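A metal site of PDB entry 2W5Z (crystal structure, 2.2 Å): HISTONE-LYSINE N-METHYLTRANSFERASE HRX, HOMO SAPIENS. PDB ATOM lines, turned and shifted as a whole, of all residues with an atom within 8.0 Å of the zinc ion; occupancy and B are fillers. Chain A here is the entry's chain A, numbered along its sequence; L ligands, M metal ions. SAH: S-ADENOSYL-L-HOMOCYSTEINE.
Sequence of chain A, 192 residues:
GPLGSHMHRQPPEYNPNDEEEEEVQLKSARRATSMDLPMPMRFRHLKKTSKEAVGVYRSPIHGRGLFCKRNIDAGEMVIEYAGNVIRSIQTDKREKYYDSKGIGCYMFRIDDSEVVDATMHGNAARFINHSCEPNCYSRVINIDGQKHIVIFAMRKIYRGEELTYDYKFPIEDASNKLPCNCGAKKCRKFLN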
ATOM      1  N   ILE A  61      11.621   2.403   8.177  1.00  0.00           N
ATOM      2  CA  ILE A  61      11.852   3.772   8.611  1.00  0.00           C
ATOM      3  C   ILE A  61      12.492   3.774   9.993  1.00  0.00           C
ATOM      4  O   ILE A  61      13.601   4.279  10.177  1.00  0.00           O
ATOM      5  CB  ILE A  61      10.541   4.605   8.623  1.00  0.00           C
ATOM      6  CG1 ILE A  61      10.019   4.762   7.191  1.00  0.00           C
ATOM      7  CG2 ILE A  61      10.769   5.971   9.239  1.00  0.00           C
ATOM      8  CD1 ILE A  61       8.615   5.370   7.076  1.00  0.00           C
ATOM      9  N   HIS A 130       7.018   9.005  11.446  1.00  0.00           N
ATOM     10  CA  HIS A 130       6.999  10.255  10.704  1.00  0.00           C
ATOM     11  C   HIS A 130       7.448  10.062   9.262  1.00  0.00           C
ATOM     12  O   HIS A 130       8.276   9.212   8.974  1.00  0.00           O
ATOM     13  CB  HIS A 130       7.900  11.298  11.360  1.00  0.00           C
ATOM     14  CG  HIS A 130       8.210  12.462  10.472  1.00  0.00           C
ATOM     15  ND1 HIS A 130       7.458  13.622  10.462  1.00  0.00           N
ATOM     16  CD2 HIS A 130       9.164  12.629   9.518  1.00  0.00           C
ATOM     17  CE1 HIS A 130       7.945  14.454   9.558  1.00  0.00           C
ATOM     18  NE2 HIS A 130       8.983  13.881   8.982  1.00  0.00           N
ATOM     19  N   SER A 131       6.897  10.876   8.369  1.00  0.00           N
ATOM     20  CA  SER A 131       7.367  10.934   6.995  1.00  0.00           C
ATOM     21  C   SER A 131       7.145  12.313   6.406  1.00  0.00           C
ATOM     22  O   SER A 131       6.119  12.944   6.633  1.00  0.00           O
ATOM     23  CB  SER A 131       6.650   9.909   6.122  1.00  0.00           C
ATOM     24  OG  SER A 131       6.865  10.235   4.753  1.00  0.00           O
ATOM     25  N   CYS A 132       8.118  12.770   5.633  1.00  0.00           N
ATOM     26  CA  CYS A 132       8.044  14.077   5.001  1.00  0.00           C
ATOM     27  C   CYS A 132       7.053  14.050   3.824  1.00  0.00           C
ATOM     28  O   CYS A 132       6.656  15.098   3.317  1.00  0.00           O
ATOM     29  CB  CYS A 132       9.430  14.523   4.555  1.00  0.00           C
ATOM     30  SG  CYS A 132      10.623  14.660   5.925  1.00  0.00           S
ATOM     31  N   GLU A 133       6.660  12.851   3.416  1.00  0.00           N
ATOM     32  CA  GLU A 133       5.625  12.659   2.389  1.00  0.00           C
ATOM     33  C   GLU A 133       4.561  11.685   2.904  1.00  0.00           C
ATOM     34  O   GLU A 133       4.515  10.535   2.469  1.00  0.00           O
ATOM     35  CB  GLU A 133       6.225  12.127   1.093  1.00  0.00           C
ATOM     36  CG  GLU A 133       7.008  13.167   0.293  1.00  0.00           C
ATOM     37  CD  GLU A 133       7.576  12.606  -0.993  1.00  0.00           C
ATOM     38  OE1 GLU A 133       8.289  13.351  -1.711  1.00  0.00           O
ATOM     39  OE2 GLU A 133       7.330  11.421  -1.294  1.00  0.00           O
ATOM     40  N   PRO A 179      17.966  13.060  12.776  1.00  0.00           N
ATOM     41  CA  PRO A 179      17.913  12.694  11.356  1.00  0.00           C
ATOM     42  C   PRO A 179      16.587  12.033  11.033  1.00  0.00           C
ATOM     43  O   PRO A 179      16.006  11.392  11.918  1.00  0.00           O
ATOM     44  CB  PRO A 179      19.054  11.686  11.202  1.00  0.00           C
ATOM     45  CG  PRO A 179      19.880  11.808  12.452  1.00  0.00           C
ATOM     46  CD  PRO A 179      18.923  12.221  13.517  1.00  0.00           C
ATOM     47  N   CYS A 180      16.108  12.192   9.806  1.00  0.00           N
ATOM     48  CA  CYS A 180      14.881  11.525   9.363  1.00  0.00           C
ATOM     49  C   CYS A 180      15.224  10.409   8.370  1.00  0.00           C
ATOM     50  O   CYS A 180      15.986  10.615   7.439  1.00  0.00           O
ATOM     51  CB  CYS A 180      13.921  12.545   8.728  1.00  0.00           C
ATOM     52  SG  CYS A 180      12.407  11.838   8.008  1.00  0.00           S
ATOM     53  N   ASN A 181      14.644   9.224   8.591  1.00  0.00           N
ATOM     54  CA  ASN A 181      14.872   8.089   7.695  1.00  0.00           C
ATOM     55  C   ASN A 181      13.679   7.763   6.787  1.00  0.00           C
ATOM     56  O   ASN A 181      13.547   6.627   6.340  1.00  0.00           O
ATOM     57  CB  ASN A 181      15.234   6.833   8.497  1.00  0.00           C
ATOM     58  CG  ASN A 181      16.207   7.104   9.637  1.00  0.00           C
ATOM     59  OD1 ASN A 181      16.095   6.520  10.717  1.00  0.00           O
ATOM     60  ND2 ASN A 181      17.168   7.984   9.398  1.00  0.00           N
ATOM     61  N   CYS A 182      12.807   8.730   6.497  1.00  0.00           N
ATOM     62  CA  CYS A 182      11.573   8.418   5.763  1.00  0.00           C
ATOM     63  C   CYS A 182      11.789   7.975   4.318  1.00  0.00           C
ATOM     64  O   CYS A 182      10.945   7.305   3.729  1.00  0.00           O
ATOM     65  CB  CYS A 182      10.539   9.554   5.839  1.00  0.00           C
ATOM     66  SG  CYS A 182      10.809  10.964   4.730  1.00  0.00           S
ATOM     67  N   GLY A 183      12.941   8.351   3.752  1.00  0.00           N
ATOM     68  CA  GLY A 183      13.313   7.893   2.423  1.00  0.00           C
ATOM     69  C   GLY A 183      12.515   8.482   1.288  1.00  0.00           C
ATOM     70  O   GLY A 183      12.566   7.981   0.164  1.00  0.00           O
ATOM     71  N   ALA A 184      11.770   9.550   1.568  1.00  0.00           N
ATOM     72  CA  ALA A 184      10.991  10.237   0.543  1.00  0.00           C
ATOM     73  C   ALA A 184      11.913  11.103  -0.303  1.00  0.00           C
ATOM     74  O   ALA A 184      12.920  11.610   0.182  1.00  0.00           O
ATOM     75  CB  ALA A 184       9.906  11.084   1.182  1.00  0.00           C
ATOM     76  N   LYS A 185      11.564  11.266  -1.584  1.00  0.00           N
ATOM     77  CA  LYS A 185      12.372  12.092  -2.477  1.00  0.00           C
ATOM     78  C   LYS A 185      12.465  13.529  -1.980  1.00  0.00           C
ATOM     79  O   LYS A 185      13.478  14.190  -2.163  1.00  0.00           O
ATOM     80  CB  LYS A 185      11.811  12.054  -3.909  1.00  0.00           C
ATOM     81  N   LYS A 186      11.408  13.995  -1.320  1.00  0.00           N
ATOM     82  CA  LYS A 186      11.358  15.366  -0.820  1.00  0.00           C
ATOM     83  C   LYS A 186      11.675  15.451   0.674  1.00  0.00           C
ATOM     84  O   LYS A 186      11.312  16.420   1.343  1.00  0.00           O
ATOM     85  CB  LYS A 186       9.988  15.981  -1.106  1.00  0.00           C
ATOM     86  N   CYS A 187      12.350  14.422   1.188  1.00  0.00           N
ATOM     87  CA  CYS A 187      12.731  14.388   2.590  1.00  0.00           C
ATOM     88  C   CYS A 187      13.328  15.724   3.020  1.00  0.00           C
ATOM     89  O   CYS A 187      13.974  16.399   2.223  1.00  0.00           O
ATOM     90  CB  CYS A 187      13.719  13.245   2.831  1.00  0.00           C
ATOM     91  SG  CYS A 187      14.156  12.941   4.557  1.00  0.00           S
ATOM     92  N   ARG A 188      13.109  16.105   4.272  1.00  0.00           N
ATOM     93  CA  ARG A 188      13.719  17.310   4.814  1.00  0.00           C
ATOM     94  C   ARG A 188      14.994  16.994   5.581  1.00  0.00           C
ATOM     95  O   ARG A 188      15.557  17.853   6.248  1.00  0.00           O
ATOM     96  CB  ARG A 188      12.750  18.031   5.750  1.00  0.00           C
ATOM     97  CG  ARG A 188      11.344  18.184   5.225  1.00  0.00           C
ATOM     98  CD  ARG A 188      10.546  19.152   6.098  1.00  0.00           C
ATOM     99  NE  ARG A 188       9.159  18.744   6.212  1.00  0.00           N
ATOM    100  CZ  ARG A 188       8.630  18.228   7.315  1.00  0.00           C
ATOM    101  NH1 ARG A 188       7.355  17.881   7.328  1.00  0.00           N
ATOM    102  NH2 ARG A 188       9.376  18.059   8.405  1.00  0.00           N
ATOM    103  N   LYS A 189      15.425  15.734   5.510  1.00  0.00           N
ATOM    104  CA  LYS A 189      16.692  15.285   6.100  1.00  0.00           C
ATOM    105  C   LYS A 189      16.694  15.225   7.633  1.00  0.00           C
ATOM    106  O   LYS A 189      17.330  14.357   8.222  1.00  0.00           O
ATOM    107  CB  LYS A 189      17.855  16.129   5.576  1.00  0.00           C
ATOM    108  N   PHE A 190      15.994  16.149   8.290  1.00  0.00           N
ATOM    109  CA  PHE A 190      15.861  16.093   9.745  1.00  0.00           C
ATOM    110  C   PHE A 190      14.406  16.098  10.187  1.00  0.00           C
ATOM    111  O   PHE A 190      13.549  16.695   9.528  1.00  0.00           O
ATOM    112  CB  PHE A 190      16.623  17.250  10.413  1.00  0.00           C
ATOM    113  CG  PHE A 190      18.044  17.384   9.954  1.00  0.00           C
ATOM    114  CD1 PHE A 190      18.415  18.381   9.072  1.00  0.00           C
ATOM    115  CD2 PHE A 190      19.011  16.488  10.397  1.00  0.00           C
ATOM    116  CE1 PHE A 190      19.720  18.504   8.650  1.00  0.00           C
ATOM    117  CE2 PHE A 190      20.317  16.596   9.977  1.00  0.00           C
ATOM    118  CZ  PHE A 190      20.670  17.607   9.097  1.00  0.00           C
ATOM    119  N   LEU A 191      14.122  15.436  11.302  1.00  0.00           N
ATOM    120  CA  LEU A 191      12.785  15.455  11.882  1.00  0.00           C
ATOM    121  C   LEU A 191      12.488  16.847  12.393  1.00  0.00           C
ATOM    122  O   LEU A 191      11.341  17.185  12.683  1.00  0.00           O
ATOM    123  CB  LEU A 191      12.684  14.446  13.036  1.00  0.00           C
ATOM    124  CG  LEU A 191      12.693  12.953  12.705  1.00  0.00           C
ATOM    125  CD1 LEU A 191      12.942  12.126  13.955  1.00  0.00           C
ATOM    126  CD2 LEU A 191      11.388  12.551  12.034  1.00  0.00           C
HETATM  127  N   SAH L   1       9.037   3.454  15.489  1.00  0.00           N
HETATM  128  CA  SAH L   1       8.580   3.848  16.818  1.00  0.00           C
HETATM  129  CB  SAH L   1       7.077   4.182  16.737  1.00  0.00           C
HETATM  130  CG  SAH L   1       6.889   5.685  16.505  1.00  0.00           C
HETATM  131  SD  SAH L   1       7.228   6.637  18.034  1.00  0.00           S
HETATM  132  C   SAH L   1       8.816   2.680  17.799  1.00  0.00           C
HETATM  133  O   SAH L   1       8.316   2.676  18.872  1.00  0.00           O
HETATM  134  OXT SAH L   1       9.398   1.509  17.313  1.00  0.00           O
HETATM  135  C5' SAH L   1       8.189   8.125  17.616  1.00  0.00           C
HETATM  136  C4' SAH L   1       9.694   7.819  17.542  1.00  0.00           C
HETATM  137  O4' SAH L   1      10.022   6.871  16.462  1.00  0.00           O
HETATM  138  C3' SAH L   1      10.473   9.099  17.224  1.00  0.00           C
HETATM  139  O3' SAH L   1      10.813   9.787  18.397  1.00  0.00           O
HETATM  140  C2' SAH L   1      11.721   8.567  16.561  1.00  0.00           C
HETATM  141  O2' SAH L   1      12.641   8.169  17.532  1.00  0.00           O
HETATM  142  C1' SAH L   1      11.234   7.346  15.785  1.00  0.00           C
HETATM  143  N9  SAH L   1      10.876   7.757  14.429  1.00  0.00           N
HETATM  144  C8  SAH L   1       9.475   7.840  13.911  1.00  0.00           C
HETATM  145  N7  SAH L   1       9.542   8.284  12.534  1.00  0.00           N
HETATM  146  C5  SAH L   1      10.955   8.483  12.162  1.00  0.00           C
HETATM  147  C6  SAH L   1      11.616   8.926  10.885  1.00  0.00           C
HETATM  148  N6  SAH L   1      10.827   9.255   9.710  1.00  0.00           N
HETATM  149  N1  SAH L   1      13.062   9.029  10.818  1.00  0.00           N
HETATM  150  C2  SAH L   1      13.894   8.684  12.024  1.00  0.00           C
HETATM  151  N3  SAH L   1      13.231   8.259  13.270  1.00  0.00           N
HETATM  152  C4  SAH L   1      11.771   8.150  13.352  1.00  0.00           C
HETATM  153 ZN    ZN M   1      11.983  12.585   5.851  1.00  0.00          ZN
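The side-chain sulfur (SG) of Cys 187 sits close to the backbone NH (N) of Lys 189 (3.2 Å).
A ring nitrogen (NE2) of His 130 sits close to the side-chain sulfur (SG) of Cys 132 (3.6 Å).
The backbone NH (N) of Cys 180 lies within hydrogen-bond range of the backbone carbonyl oxygen (O) of Lys 189 (2.9 Å).
SG of Cys 182 sits close to N of Ala 184.
The side-chain sulfur (SG) of Cys 132 sits close to the backbone NH (N) of Arg 188 (3.3 Å).
SG of Cys 180 lies close to N6 of the ligand, at 3.5 Å.
O of His 130 sits at hydrogen-bond distance from N6 of the ligand.
A nitrogen (N1) of the ligand lies within hydrogen-bond range of the backbone NH (N) of Asn 181 (2.7 Å).
A nitrogen (N7) of the ligand sits at hydrogen-bond distance from the backbone NH of His 130 (2.8 Å).
The zinc ion is bound by SG of Cys 182 (2.3 Å).
The zinc ion is bound by SG of Cys 180.
The side-chain sulfur (SG) of Cys 132 binds the zinc ion (2.5 Å).
SG of Cys 187 is bound to the zinc ion (2.6 Å).
Within 4 Å of the zinc ion: Cys 132, Cys 180, Cys 182 and Cys 187.
The nearest printed residue that does not touch the zinc ion is Arg 188 (4.02 Å).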
